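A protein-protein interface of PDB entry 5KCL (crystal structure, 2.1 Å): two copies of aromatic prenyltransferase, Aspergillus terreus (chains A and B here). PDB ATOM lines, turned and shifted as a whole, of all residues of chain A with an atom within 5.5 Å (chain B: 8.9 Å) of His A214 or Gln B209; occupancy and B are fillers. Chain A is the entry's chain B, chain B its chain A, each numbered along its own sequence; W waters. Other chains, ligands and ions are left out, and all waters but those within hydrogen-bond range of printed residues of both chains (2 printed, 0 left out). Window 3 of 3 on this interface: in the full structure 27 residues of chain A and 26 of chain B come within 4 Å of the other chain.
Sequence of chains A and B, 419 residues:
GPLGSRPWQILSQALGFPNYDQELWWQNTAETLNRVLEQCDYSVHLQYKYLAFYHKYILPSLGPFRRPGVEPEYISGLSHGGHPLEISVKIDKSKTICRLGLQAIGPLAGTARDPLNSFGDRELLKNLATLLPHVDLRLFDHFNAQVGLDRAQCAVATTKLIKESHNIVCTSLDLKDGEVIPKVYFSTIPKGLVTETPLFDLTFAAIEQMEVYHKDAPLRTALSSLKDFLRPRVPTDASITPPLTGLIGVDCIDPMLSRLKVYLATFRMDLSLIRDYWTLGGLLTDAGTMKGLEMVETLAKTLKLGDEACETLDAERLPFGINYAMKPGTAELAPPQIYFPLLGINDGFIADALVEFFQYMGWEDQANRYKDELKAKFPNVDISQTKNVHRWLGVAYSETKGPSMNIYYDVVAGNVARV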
ATOM      1  N   GLN A 146      -2.094 -16.735 -28.048  1.00  0.00           N
ATOM      2  CA  GLN A 146      -1.786 -17.059 -26.658  1.00  0.00           C
ATOM      3  C   GLN A 146      -0.630 -16.250 -26.065  1.00  0.00           C
ATOM      4  O   GLN A 146      -0.693 -15.943 -24.903  1.00  0.00           O
ATOM      5  CB  GLN A 146      -1.521 -18.570 -26.466  1.00  0.00           C
ATOM      6  CG  GLN A 146      -2.615 -19.506 -26.975  1.00  0.00           C
ATOM      7  CD  GLN A 146      -3.991 -19.249 -26.414  1.00  0.00           C
ATOM      8  OE1 GLN A 146      -4.991 -19.071 -27.156  1.00  0.00           O
ATOM      9  NE2 GLN A 146      -4.075 -19.307 -25.117  1.00  0.00           N
ATOM     10  N   GLU A 208      -2.266 -26.385 -23.734  1.00  0.00           N
ATOM     11  CA  GLU A 208      -3.471 -27.146 -23.369  1.00  0.00           C
ATOM     12  C   GLU A 208      -4.748 -26.577 -23.982  1.00  0.00           C
ATOM     13  O   GLU A 208      -5.732 -27.272 -24.068  1.00  0.00           O
ATOM     14  CB  GLU A 208      -3.568 -27.207 -21.846  1.00  0.00           C
ATOM     15  CG  GLU A 208      -2.555 -28.210 -21.268  1.00  0.00           C
ATOM     16  CD  GLU A 208      -2.212 -28.071 -19.778  1.00  0.00           C
ATOM     17  OE1 GLU A 208      -1.113 -28.527 -19.328  1.00  0.00           O
ATOM     18  OE2 GLU A 208      -3.029 -27.483 -19.053  1.00  0.00           O
ATOM     19  N   GLN A 209      -4.701 -25.348 -24.484  1.00  0.00           N
ATOM     20  CA  GLN A 209      -5.798 -24.803 -25.288  1.00  0.00           C
ATOM     21  C   GLN A 209      -5.715 -25.096 -26.805  1.00  0.00           C
ATOM     22  O   GLN A 209      -6.614 -24.747 -27.492  1.00  0.00           O
ATOM     23  CB  GLN A 209      -5.965 -23.319 -24.995  1.00  0.00           C
ATOM     24  CG  GLN A 209      -6.658 -23.096 -23.660  1.00  0.00           C
ATOM     25  CD  GLN A 209      -6.046 -21.976 -22.848  1.00  0.00           C
ATOM     26  OE1 GLN A 209      -5.685 -22.171 -21.669  1.00  0.00           O
ATOM     27  NE2 GLN A 209      -5.959 -20.784 -23.447  1.00  0.00           N
ATOM     28  N   MET A 210      -4.681 -25.801 -27.289  1.00  0.00           N
ATOM     29  CA  MET A 210      -4.606 -26.202 -28.702  1.00  0.00           C
ATOM     30  C   MET A 210      -5.744 -27.144 -29.062  1.00  0.00           C
ATOM     31  O   MET A 210      -6.014 -28.095 -28.304  1.00  0.00           O
ATOM     32  CB  MET A 210      -3.329 -26.993 -29.002  1.00  0.00           C
ATOM     33  CG  MET A 210      -2.030 -26.225 -28.997  1.00  0.00           C
ATOM     34  SD  MET A 210      -0.598 -27.331 -28.974  1.00  0.00           S
ATOM     35  CE  MET A 210      -0.271 -27.624 -30.690  1.00  0.00           C
ATOM     36  N   GLU A 211      -6.336 -26.949 -30.241  1.00  0.00           N
ATOM     37  CA  GLU A 211      -7.326 -27.890 -30.773  1.00  0.00           C
ATOM     38  C   GLU A 211      -6.807 -29.340 -30.826  1.00  0.00           C
ATOM     39  O   GLU A 211      -7.505 -30.253 -30.409  1.00  0.00           O
ATOM     40  CB  GLU A 211      -7.840 -27.447 -32.140  1.00  0.00           C
ATOM     41  CG  GLU A 211      -8.745 -28.465 -32.830  1.00  0.00           C
ATOM     42  CD  GLU A 211      -9.453 -27.922 -34.062  1.00  0.00           C
ATOM     43  OE1 GLU A 211      -8.987 -26.908 -34.613  1.00  0.00           O
ATOM     44  OE2 GLU A 211     -10.478 -28.505 -34.487  1.00  0.00           O
ATOM     45  N   VAL A 212      -5.571 -29.545 -31.252  1.00  0.00           N
ATOM     46  CA  VAL A 212      -5.000 -30.927 -31.277  1.00  0.00           C
ATOM     47  C   VAL A 212      -4.826 -31.574 -29.888  1.00  0.00           C
ATOM     48  O   VAL A 212      -4.992 -32.792 -29.739  1.00  0.00           O
ATOM     49  CB  VAL A 212      -3.663 -31.012 -32.028  1.00  0.00           C
ATOM     50  CG1 VAL A 212      -3.859 -30.587 -33.463  1.00  0.00           C
ATOM     51  CG2 VAL A 212      -2.636 -30.101 -31.410  1.00  0.00           C
ATOM     52  N   TYR A 213      -4.498 -30.760 -28.882  1.00  0.00           N
ATOM     53  CA  TYR A 213      -4.413 -31.258 -27.526  1.00  0.00           C
ATOM     54  C   TYR A 213      -5.748 -31.871 -27.118  1.00  0.00           C
ATOM     55  O   TYR A 213      -5.761 -32.940 -26.497  1.00  0.00           O
ATOM     56  CB  TYR A 213      -4.002 -30.151 -26.577  1.00  0.00           C
ATOM     57  CG  TYR A 213      -3.887 -30.558 -25.118  1.00  0.00           C
ATOM     58  CD1 TYR A 213      -5.001 -30.486 -24.250  1.00  0.00           C
ATOM     59  CD2 TYR A 213      -2.677 -30.970 -24.581  1.00  0.00           C
ATOM     60  CE1 TYR A 213      -4.882 -30.832 -22.892  1.00  0.00           C
ATOM     61  CE2 TYR A 213      -2.550 -31.306 -23.243  1.00  0.00           C
ATOM     62  CZ  TYR A 213      -3.643 -31.244 -22.405  1.00  0.00           C
ATOM     63  OH  TYR A 213      -3.491 -31.591 -21.107  1.00  0.00           O
ATOM     64  N   HIS A 214      -6.850 -31.182 -27.429  1.00  0.00           N
ATOM     65  CA  HIS A 214      -8.194 -31.675 -27.076  1.00  0.00           C
ATOM     66  C   HIS A 214      -8.623 -32.935 -27.830  1.00  0.00           C
ATOM     67  O   HIS A 214      -9.385 -33.701 -27.310  1.00  0.00           O
ATOM     68  CB  HIS A 214      -9.232 -30.550 -27.213  1.00  0.00           C
ATOM     69  CG  HIS A 214      -9.133 -29.527 -26.123  1.00  0.00           C
ATOM     70  ND1 HIS A 214     -10.040 -29.449 -25.086  1.00  0.00           N
ATOM     71  CD2 HIS A 214      -8.197 -28.574 -25.875  1.00  0.00           C
ATOM     72  CE1 HIS A 214      -9.678 -28.482 -24.256  1.00  0.00           C
ATOM     73  NE2 HIS A 214      -8.559 -27.939 -24.708  1.00  0.00           N
ATOM     74  N   LYS A 215      -8.099 -33.168 -29.024  1.00  0.00           N
ATOM     75  CA  LYS A 215      -8.382 -34.372 -29.793  1.00  0.00           C
ATOM     76  C   LYS A 215      -7.422 -35.554 -29.608  1.00  0.00           C
ATOM     77  O   LYS A 215      -7.741 -36.648 -30.039  1.00  0.00           O
ATOM     78  CB  LYS A 215      -8.358 -34.029 -31.288  1.00  0.00           C
ATOM     79  CG  LYS A 215      -9.387 -33.005 -31.700  1.00  0.00           C
ATOM     80  CD  LYS A 215      -9.465 -32.871 -33.209  1.00  0.00           C
ATOM     81  CE  LYS A 215     -10.483 -31.806 -33.578  1.00  0.00           C
ATOM     82  NZ  LYS A 215     -10.183 -31.285 -34.935  1.00  0.00           N
ATOM     83  N   ASP A 216      -6.226 -35.345 -29.073  1.00  0.00           N
ATOM     84  CA  ASP A 216      -5.198 -36.409 -29.076  1.00  0.00           C
ATOM     85  C   ASP A 216      -4.752 -36.819 -27.656  1.00  0.00           C
ATOM     86  O   ASP A 216      -3.921 -36.166 -27.034  1.00  0.00           O
ATOM     87  CB  ASP A 216      -4.024 -35.968 -29.928  1.00  0.00           C
ATOM     88  CG  ASP A 216      -3.198 -37.124 -30.418  1.00  0.00           C
ATOM     89  OD1 ASP A 216      -3.615 -37.777 -31.382  1.00  0.00           O
ATOM     90  OD2 ASP A 216      -2.101 -37.361 -29.883  1.00  0.00           O
ATOM     91  N   ARG A 220      -1.587 -35.651 -24.941  1.00  0.00           N
ATOM     92  CA  ARG A 220      -1.889 -35.183 -23.548  1.00  0.00           C
ATOM     93  C   ARG A 220      -1.068 -35.993 -22.521  1.00  0.00           C
ATOM     94  O   ARG A 220      -0.468 -35.419 -21.617  1.00  0.00           O
ATOM     95  CB  ARG A 220      -3.369 -35.241 -23.221  1.00  0.00           C
ATOM     96  CG  ARG A 220      -4.257 -34.379 -24.122  1.00  0.00           C
ATOM     97  CD  ARG A 220      -5.610 -34.041 -23.476  1.00  0.00           C
ATOM     98  NE  ARG A 220      -6.426 -35.237 -23.339  1.00  0.00           N
ATOM     99  CZ  ARG A 220      -7.115 -35.836 -24.312  1.00  0.00           C
ATOM    100  NH1 ARG A 220      -7.149 -35.366 -25.553  1.00  0.00           N
ATOM    101  NH2 ARG A 220      -7.799 -36.940 -24.027  1.00  0.00           N
ATOM    102  N   LEU B 139      -7.863 -12.111 -30.426  1.00  0.00           N
ATOM    103  CA  LEU B 139      -9.101 -12.826 -30.676  1.00  0.00           C
ATOM    104  C   LEU B 139      -9.255 -13.167 -32.151  1.00  0.00           C
ATOM    105  O   LEU B 139      -9.739 -14.257 -32.495  1.00  0.00           O
ATOM    106  CB  LEU B 139     -10.310 -12.050 -30.167  1.00  0.00           C
ATOM    107  CG  LEU B 139     -10.406 -12.020 -28.634  1.00  0.00           C
ATOM    108  CD1 LEU B 139     -11.585 -11.159 -28.261  1.00  0.00           C
ATOM    109  CD2 LEU B 139     -10.568 -13.374 -27.981  1.00  0.00           C
ATOM    110  N   HIS B 142      -7.047 -16.156 -32.579  1.00  0.00           N
ATOM    111  CA  HIS B 142      -7.627 -17.331 -31.926  1.00  0.00           C
ATOM    112  C   HIS B 142      -8.671 -17.975 -32.808  1.00  0.00           C
ATOM    113  O   HIS B 142      -8.609 -19.166 -33.063  1.00  0.00           O
ATOM    114  CB  HIS B 142      -8.287 -16.999 -30.560  1.00  0.00           C
ATOM    115  CG  HIS B 142      -9.027 -18.166 -30.013  1.00  0.00           C
ATOM    116  ND1 HIS B 142      -8.385 -19.215 -29.387  1.00  0.00           N
ATOM    117  CD2 HIS B 142     -10.347 -18.492 -30.054  1.00  0.00           C
ATOM    118  CE1 HIS B 142      -9.282 -20.120 -29.019  1.00  0.00           C
ATOM    119  NE2 HIS B 142     -10.472 -19.729 -29.455  1.00  0.00           N
ATOM    120  N   PHE B 143      -9.652 -17.196 -33.260  1.00  0.00           N
ATOM    121  CA  PHE B 143     -10.716 -17.786 -34.058  1.00  0.00           C
ATOM    122  C   PHE B 143     -10.283 -18.206 -35.435  1.00  0.00           C
ATOM    123  O   PHE B 143     -10.826 -19.155 -35.966  1.00  0.00           O
ATOM    124  CB  PHE B 143     -11.950 -16.891 -34.091  1.00  0.00           C
ATOM    125  CG  PHE B 143     -12.712 -16.962 -32.813  1.00  0.00           C
ATOM    126  CD1 PHE B 143     -13.449 -18.124 -32.509  1.00  0.00           C
ATOM    127  CD2 PHE B 143     -12.585 -15.976 -31.864  1.00  0.00           C
ATOM    128  CE1 PHE B 143     -14.123 -18.224 -31.318  1.00  0.00           C
ATOM    129  CE2 PHE B 143     -13.260 -16.078 -30.651  1.00  0.00           C
ATOM    130  CZ  PHE B 143     -13.995 -17.217 -30.374  1.00  0.00           C
ATOM    131  N   ALA B 145      -7.470 -19.566 -35.989  1.00  0.00           N
ATOM    132  CA  ALA B 145      -6.903 -20.896 -35.743  1.00  0.00           C
ATOM    133  C   ALA B 145      -7.990 -21.948 -35.574  1.00  0.00           C
ATOM    134  O   ALA B 145      -7.828 -23.073 -36.057  1.00  0.00           O
ATOM    135  CB  ALA B 145      -6.001 -20.906 -34.521  1.00  0.00           C
ATOM    136  N   GLN B 146      -9.098 -21.593 -34.941  1.00  0.00           N
ATOM    137  CA  GLN B 146     -10.151 -22.563 -34.663  1.00  0.00           C
ATOM    138  C   GLN B 146     -11.091 -22.857 -35.810  1.00  0.00           C
ATOM    139  O   GLN B 146     -11.522 -23.999 -35.941  1.00  0.00           O
ATOM    140  CB  GLN B 146     -11.009 -22.105 -33.499  1.00  0.00           C
ATOM    141  CG  GLN B 146     -10.283 -21.821 -32.227  1.00  0.00           C
ATOM    142  CD  GLN B 146      -9.411 -22.967 -31.706  1.00  0.00           C
ATOM    143  OE1 GLN B 146      -8.204 -22.810 -31.466  1.00  0.00           O
ATOM    144  NE2 GLN B 146     -10.031 -24.080 -31.495  1.00  0.00           N
ATOM    145  N   VAL B 147     -11.428 -21.876 -36.645  1.00  0.00           N
ATOM    146  CA  VAL B 147     -12.435 -22.071 -37.682  1.00  0.00           C
ATOM    147  C   VAL B 147     -11.832 -21.964 -39.103  1.00  0.00           C
ATOM    148  O   VAL B 147     -12.524 -22.147 -40.102  1.00  0.00           O
ATOM    149  CB  VAL B 147     -13.577 -21.059 -37.365  1.00  0.00           C
ATOM    150  CG1 VAL B 147     -14.607 -20.921 -38.441  1.00  0.00           C
ATOM    151  CG2 VAL B 147     -14.266 -21.483 -36.082  1.00  0.00           C
ATOM    152  N   LYS B 191     -16.061 -24.804 -42.103  1.00  0.00           N
ATOM    153  CA  LYS B 191     -15.479 -25.847 -41.246  1.00  0.00           C
ATOM    154  C   LYS B 191     -16.504 -26.967 -40.916  1.00  0.00           C
ATOM    155  O   LYS B 191     -16.152 -28.117 -41.009  1.00  0.00           O
ATOM    156  CB  LYS B 191     -14.889 -25.276 -39.974  1.00  0.00           C
ATOM    157  CG  LYS B 191     -13.835 -26.207 -39.414  1.00  0.00           C
ATOM    158  CD  LYS B 191     -13.581 -26.039 -37.934  1.00  0.00           C
ATOM    159  CE  LYS B 191     -12.399 -26.937 -37.516  1.00  0.00           C
ATOM    160  NZ  LYS B 191     -12.029 -26.693 -36.093  1.00  0.00           N
ATOM    161  N   ASP B 201     -21.586 -27.728 -32.187  1.00  0.00           N
ATOM    162  CA  ASP B 201     -20.384 -28.230 -31.501  1.00  0.00           C
ATOM    163  C   ASP B 201     -19.135 -27.419 -31.850  1.00  0.00           C
ATOM    164  O   ASP B 201     -18.267 -27.148 -31.008  1.00  0.00           O
ATOM    165  CB  ASP B 201     -20.047 -29.704 -31.874  1.00  0.00           C
ATOM    166  CG  ASP B 201     -21.116 -30.712 -31.434  1.00  0.00           C
ATOM    167  OD1 ASP B 201     -22.022 -30.376 -30.655  1.00  0.00           O
ATOM    168  OD2 ASP B 201     -21.030 -31.861 -31.900  1.00  0.00           O
ATOM    169  N   LEU B 202     -18.927 -27.148 -33.130  1.00  0.00           N
ATOM    170  CA  LEU B 202     -17.660 -26.449 -33.457  1.00  0.00           C
ATOM    171  C   LEU B 202     -17.658 -25.014 -32.950  1.00  0.00           C
ATOM    172  O   LEU B 202     -16.624 -24.565 -32.556  1.00  0.00           O
ATOM    173  CB  LEU B 202     -17.225 -26.577 -34.920  1.00  0.00           C
ATOM    174  CG  LEU B 202     -17.934 -25.851 -36.051  1.00  0.00           C
ATOM    175  CD1 LEU B 202     -17.161 -24.563 -36.310  1.00  0.00           C
ATOM    176  CD2 LEU B 202     -17.956 -26.726 -37.323  1.00  0.00           C
ATOM    177  N   THR B 203     -18.807 -24.342 -32.933  1.00  0.00           N
ATOM    178  CA  THR B 203     -18.928 -22.980 -32.426  1.00  0.00           C
ATOM    179  C   THR B 203     -18.512 -22.905 -30.973  1.00  0.00           C
ATOM    180  O   THR B 203     -17.629 -22.165 -30.617  1.00  0.00           O
ATOM    181  CB  THR B 203     -20.352 -22.441 -32.592  1.00  0.00           C
ATOM    182  OG1 THR B 203     -20.606 -22.338 -33.964  1.00  0.00           O
ATOM    183  CG2 THR B 203     -20.527 -21.050 -31.996  1.00  0.00           C
ATOM    184  N   PHE B 204     -19.110 -23.768 -30.159  1.00  0.00           N
ATOM    185  CA  PHE B 204     -18.792 -23.814 -28.736  1.00  0.00           C
ATOM    186  C   PHE B 204     -17.435 -24.394 -28.466  1.00  0.00           C
ATOM    187  O   PHE B 204     -16.787 -23.958 -27.535  1.00  0.00           O
ATOM    188  CB  PHE B 204     -19.978 -24.385 -27.897  1.00  0.00           C
ATOM    189  CG  PHE B 204     -21.134 -23.439 -27.881  1.00  0.00           C
ATOM    190  CD1 PHE B 204     -21.064 -22.281 -27.111  1.00  0.00           C
ATOM    191  CD2 PHE B 204     -22.185 -23.578 -28.760  1.00  0.00           C
ATOM    192  CE1 PHE B 204     -22.076 -21.342 -27.156  1.00  0.00           C
ATOM    193  CE2 PHE B 204     -23.214 -22.656 -28.806  1.00  0.00           C
ATOM    194  CZ  PHE B 204     -23.142 -21.517 -28.002  1.00  0.00           C
ATOM    195  N   ALA B 205     -16.977 -25.338 -29.262  1.00  0.00           N
ATOM    196  CA  ALA B 205     -15.610 -25.849 -29.041  1.00  0.00           C
ATOM    197  C   ALA B 205     -14.589 -24.696 -29.213  1.00  0.00           C
ATOM    198  O   ALA B 205     -13.696 -24.500 -28.386  1.00  0.00           O
ATOM    199  CB  ALA B 205     -15.318 -27.038 -29.985  1.00  0.00           C
ATOM    200  N   ALA B 206     -14.771 -23.874 -30.256  1.00  0.00           N
ATOM    201  CA  ALA B 206     -13.846 -22.757 -30.500  1.00  0.00           C
ATOM    202  C   ALA B 206     -13.910 -21.695 -29.385  1.00  0.00           C
ATOM    203  O   ALA B 206     -12.872 -21.222 -28.888  1.00  0.00           O
ATOM    204  CB  ALA B 206     -14.136 -22.114 -31.833  1.00  0.00           C
ATOM    205  N   ILE B 207     -15.115 -21.366 -28.963  1.00  0.00           N
ATOM    206  CA  ILE B 207     -15.268 -20.459 -27.818  1.00  0.00           C
ATOM    207  C   ILE B 207     -14.659 -20.945 -26.538  1.00  0.00           C
ATOM    208  O   ILE B 207     -14.041 -20.177 -25.821  1.00  0.00           O
ATOM    209  CB  ILE B 207     -16.753 -20.119 -27.568  1.00  0.00           C
ATOM    210  CG1 ILE B 207     -17.270 -19.286 -28.749  1.00  0.00           C
ATOM    211  CG2 ILE B 207     -16.918 -19.365 -26.249  1.00  0.00           C
ATOM    212  CD1 ILE B 207     -18.775 -19.227 -28.869  1.00  0.00           C
ATOM    213  N   GLU B 208     -14.825 -22.227 -26.238  1.00  0.00           N
ATOM    214  CA  GLU B 208     -14.361 -22.769 -24.970  1.00  0.00           C
ATOM    215  C   GLU B 208     -12.841 -22.898 -24.893  1.00  0.00           C
ATOM    216  O   GLU B 208     -12.287 -23.059 -23.802  1.00  0.00           O
ATOM    217  CB  GLU B 208     -15.053 -24.107 -24.702  1.00  0.00           C
ATOM    218  CG  GLU B 208     -16.483 -23.871 -24.245  1.00  0.00           C
ATOM    219  CD  GLU B 208     -17.407 -25.054 -24.450  1.00  0.00           C
ATOM    220  OE1 GLU B 208     -16.903 -26.183 -24.540  1.00  0.00           O
ATOM    221  OE2 GLU B 208     -18.639 -24.827 -24.515  1.00  0.00           O
ATOM    222  N   GLN B 209     -12.163 -22.821 -26.035  1.00  0.00           N
ATOM    223  CA  GLN B 209     -10.722 -22.807 -26.004  1.00  0.00           C
ATOM    224  C   GLN B 209     -10.121 -21.421 -25.917  1.00  0.00           C
ATOM    225  O   GLN B 209      -8.927 -21.316 -25.840  1.00  0.00           O
ATOM    226  CB  GLN B 209     -10.166 -23.659 -27.161  1.00  0.00           C
ATOM    227  CG  GLN B 209     -10.254 -25.165 -26.852  1.00  0.00           C
ATOM    228  CD  GLN B 209     -10.724 -26.000 -28.025  1.00  0.00           C
ATOM    229  OE1 GLN B 209     -11.717 -26.766 -27.927  1.00  0.00           O
ATOM    230  NE2 GLN B 209     -10.023 -25.854 -29.170  1.00  0.00           N
ATOM    231  N   MET B 210     -10.929 -20.357 -25.906  1.00  0.00           N
ATOM    232  CA  MET B 210     -10.417 -18.980 -25.713  1.00  0.00           C
ATOM    233  C   MET B 210      -9.686 -18.813 -24.405  1.00  0.00           C
ATOM    234  O   MET B 210     -10.199 -19.272 -23.371  1.00  0.00           O
ATOM    235  CB  MET B 210     -11.543 -17.936 -25.660  1.00  0.00           C
ATOM    236  CG  MET B 210     -12.276 -17.646 -26.940  1.00  0.00           C
ATOM    237  SD  MET B 210     -13.826 -16.751 -26.692  1.00  0.00           S
ATOM    238  CE  MET B 210     -13.307 -15.037 -26.744  1.00  0.00           C
ATOM    239  N   GLU B 211      -8.555 -18.097 -24.428  1.00  0.00           N
ATOM    240  CA  GLU B 211      -7.841 -17.710 -23.187  1.00  0.00           C
ATOM    241  C   GLU B 211      -8.769 -16.989 -22.182  1.00  0.00           C
ATOM    242  O   GLU B 211      -8.760 -17.346 -21.020  1.00  0.00           O
ATOM    243  CB  GLU B 211      -6.568 -16.902 -23.465  1.00  0.00           C
ATOM    244  CG  GLU B 211      -5.896 -16.360 -22.225  1.00  0.00           C
ATOM    245  CD  GLU B 211      -4.536 -15.692 -22.430  1.00  0.00           C
ATOM    246  OE1 GLU B 211      -3.744 -15.662 -21.465  1.00  0.00           O
ATOM    247  OE2 GLU B 211      -4.247 -15.131 -23.516  1.00  0.00           O
ATOM    248  N   VAL B 212      -9.593 -16.046 -22.643  1.00  0.00           N
ATOM    249  CA  VAL B 212     -10.506 -15.353 -21.741  1.00  0.00           C
ATOM    250  C   VAL B 212     -11.588 -16.279 -21.125  1.00  0.00           C
ATOM    251  O   VAL B 212     -11.949 -16.098 -19.960  1.00  0.00           O
ATOM    252  CB  VAL B 212     -11.190 -14.140 -22.369  1.00  0.00           C
ATOM    253  CG1 VAL B 212     -12.160 -13.517 -21.359  1.00  0.00           C
ATOM    254  CG2 VAL B 212     -10.161 -13.086 -22.711  1.00  0.00           C
ATOM    255  N   TYR B 213     -12.080 -17.250 -21.887  1.00  0.00           N
ATOM    256  CA  TYR B 213     -12.989 -18.252 -21.349  1.00  0.00           C
ATOM    257  C   TYR B 213     -12.385 -18.964 -20.144  1.00  0.00           C
ATOM    258  O   TYR B 213     -13.054 -19.115 -19.127  1.00  0.00           O
ATOM    259  CB  TYR B 213     -13.386 -19.286 -22.411  1.00  0.00           C
ATOM    260  CG  TYR B 213     -14.352 -20.358 -21.965  1.00  0.00           C
ATOM    261  CD1 TYR B 213     -13.910 -21.542 -21.405  1.00  0.00           C
ATOM    262  CD2 TYR B 213     -15.714 -20.179 -22.129  1.00  0.00           C
ATOM    263  CE1 TYR B 213     -14.821 -22.518 -21.005  1.00  0.00           C
ATOM    264  CE2 TYR B 213     -16.619 -21.150 -21.769  1.00  0.00           C
ATOM    265  CZ  TYR B 213     -16.172 -22.292 -21.178  1.00  0.00           C
ATOM    266  OH  TYR B 213     -17.111 -23.244 -20.809  1.00  0.00           O
ATOM    267  N   HIS B 214     -11.127 -19.374 -20.248  1.00  0.00           N
ATOM    268  CA  HIS B 214     -10.413 -20.026 -19.114  1.00  0.00           C
ATOM    269  C   HIS B 214     -10.170 -19.127 -17.894  1.00  0.00           C
ATOM    270  O   HIS B 214     -10.105 -19.635 -16.812  1.00  0.00           O
ATOM    271  CB  HIS B 214      -9.119 -20.690 -19.612  1.00  0.00           C
ATOM    272  CG  HIS B 214      -9.386 -21.925 -20.425  1.00  0.00           C
ATOM    273  ND1 HIS B 214      -9.171 -23.203 -19.940  1.00  0.00           N
ATOM    274  CD2 HIS B 214      -9.918 -22.082 -21.660  1.00  0.00           C
ATOM    275  CE1 HIS B 214      -9.546 -24.092 -20.850  1.00  0.00           C
ATOM    276  NE2 HIS B 214     -10.004 -23.435 -21.903  1.00  0.00           N
ATOM    277  N   LYS B 215     -10.072 -17.803 -18.070  1.00  0.00           N
ATOM    278  CA  LYS B 215      -9.863 -16.852 -16.964  1.00  0.00           C
ATOM    279  C   LYS B 215     -11.138 -16.231 -16.378  1.00  0.00           C
ATOM    280  O   LYS B 215     -11.062 -15.639 -15.324  1.00  0.00           O
ATOM    281  CB  LYS B 215      -8.996 -15.674 -17.420  1.00  0.00           C
ATOM    282  CG  LYS B 215      -7.613 -16.092 -17.858  1.00  0.00           C
ATOM    283  CD  LYS B 215      -6.717 -14.897 -18.104  1.00  0.00           C
ATOM    284  CE  LYS B 215      -5.350 -15.364 -18.581  1.00  0.00           C
ATOM    285  NZ  LYS B 215      -4.683 -14.264 -19.322  1.00  0.00           N
ATOM    286  N   ARG B 220     -17.988 -17.776 -18.807  1.00  0.00           N
ATOM    287  CA  ARG B 220     -18.338 -19.201 -18.904  1.00  0.00           C
ATOM    288  C   ARG B 220     -19.818 -19.431 -18.520  1.00  0.00           C
ATOM    289  O   ARG B 220     -20.539 -20.218 -19.138  1.00  0.00           O
ATOM    290  CB  ARG B 220     -17.432 -20.086 -18.039  1.00  0.00           C
ATOM    291  CG  ARG B 220     -15.954 -19.996 -18.403  1.00  0.00           C
ATOM    292  CD  ARG B 220     -15.155 -21.229 -17.951  1.00  0.00           C
ATOM    293  NE  ARG B 220     -15.074 -21.270 -16.505  1.00  0.00           N
ATOM    294  CZ  ARG B 220     -14.256 -20.553 -15.741  1.00  0.00           C
ATOM    295  NH1 ARG B 220     -13.361 -19.690 -16.260  1.00  0.00           N
ATOM    296  NH2 ARG B 220     -14.330 -20.694 -14.414  1.00  0.00           N
HETATM  297  O   HOH W   1      -5.526 -24.608 -31.699  1.00  0.00           O
HETATM  298  O   HOH W   2      -7.371 -17.560 -26.985  1.00  0.00           O
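Of the 23 printed residues of chain B, 4 touch a printed residue of chain A. Of the 11 printed residues of chain A, 4 touch a printed residue of chain B. Printed residues of chain A that touch a printed residue of chain B: Gln A146, Gln A209, Glu A211 and His A214. Hydrophobic or aromatic side chains of chain A that line the printed part of chain B: His A214. Among the printed residues, 7 pairs touch across the chains. Among the printed residues, Asp or Glu carboxylates within 4 Å of a Lys or Arg side-chain nitrogen of the other chain: Glu A211 with Lys B191.
The side-chain amino group of Lys B191 is in salt-bridge range of the side-chain carboxylate of Glu A211 (2.9 Å).
Of the printed residues of chain B, Gln A209 touches Gln B209, Glu B211 and His B214. Of chain B, only Gln B209 comes within 4 Å of His A214. Phe B143 touches none of the printed residues of chain A. Ala B206 touches none of the printed residues of chain A. Gln B209 touches just these residues of chain A: Gln A209, Glu A211 and His A214. Of the printed residues of chain A, Glu B211 touches Gln A146 and Gln A209.
The side-chain amino group of Lys B191 is in hydrogen-bond range of the backbone carbonyl oxygen of Gln B146, at 2.7 Å. The side-chain amide nitrogen (NE2) of Gln B209 lies close to the side-chain amide nitrogen (NE2) of Gln B146 (2.9 Å). O of Ala B205 sits close to OE1 of Gln B209 (3.0 Å). The side-chain carboxylate (OE1) of Glu B211 lies within salt-bridge range of the side-chain amino group (NZ) of Lys B215 (2.7 Å). The side-chain amide nitrogen of Gln A209 sits close to the side-chain amide nitrogen of Gln A146, at 2.9 Å. NZ of Lys A215 is in salt-bridge range of OE2 of Glu A211, at 2.8 Å.
Gln A146 touches Glu B211, but with the chains exchanged Glu A211 does not touch Gln B146 (4.1 Å). Gln B209 touches its own counterpart, Gln A209. Gln A209 touches Glu B211, and with the chains exchanged Glu A211 touches Gln B209. Gln A209 touches His B214, and with the chains exchanged His A214 touches Gln B209. Positions printed for both chains: 146, 208, 209, 210, 211, 212, 213, 214, 215 and 220.
Gln A146 touches Glu B211 (NE2 to CB, 3.8 Å). CG of Gln A209 touches O of Gln B209, 3.6 Å away. Glu B211 touches Gln A209. CG of Gln A209 touches NE2 of His B214, at 3.8 Å. Glu A211 touches Gln B209 (CA to NE2, 3.7 Å). Gln B209 touches His A214 (CG to NE2, 3.9 Å).
Water W2 lies within hydrogen-bond range of the side-chain amide oxygen of Gln A146, the backbone NH of Glu B211 and a ring nitrogen (ND1) of His B142. Water W1 lies within hydrogen-bond range of the backbone NH of Glu A211 (2.9 Å) and the side-chain amide oxygen of Gln B146 (3.2 Å).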
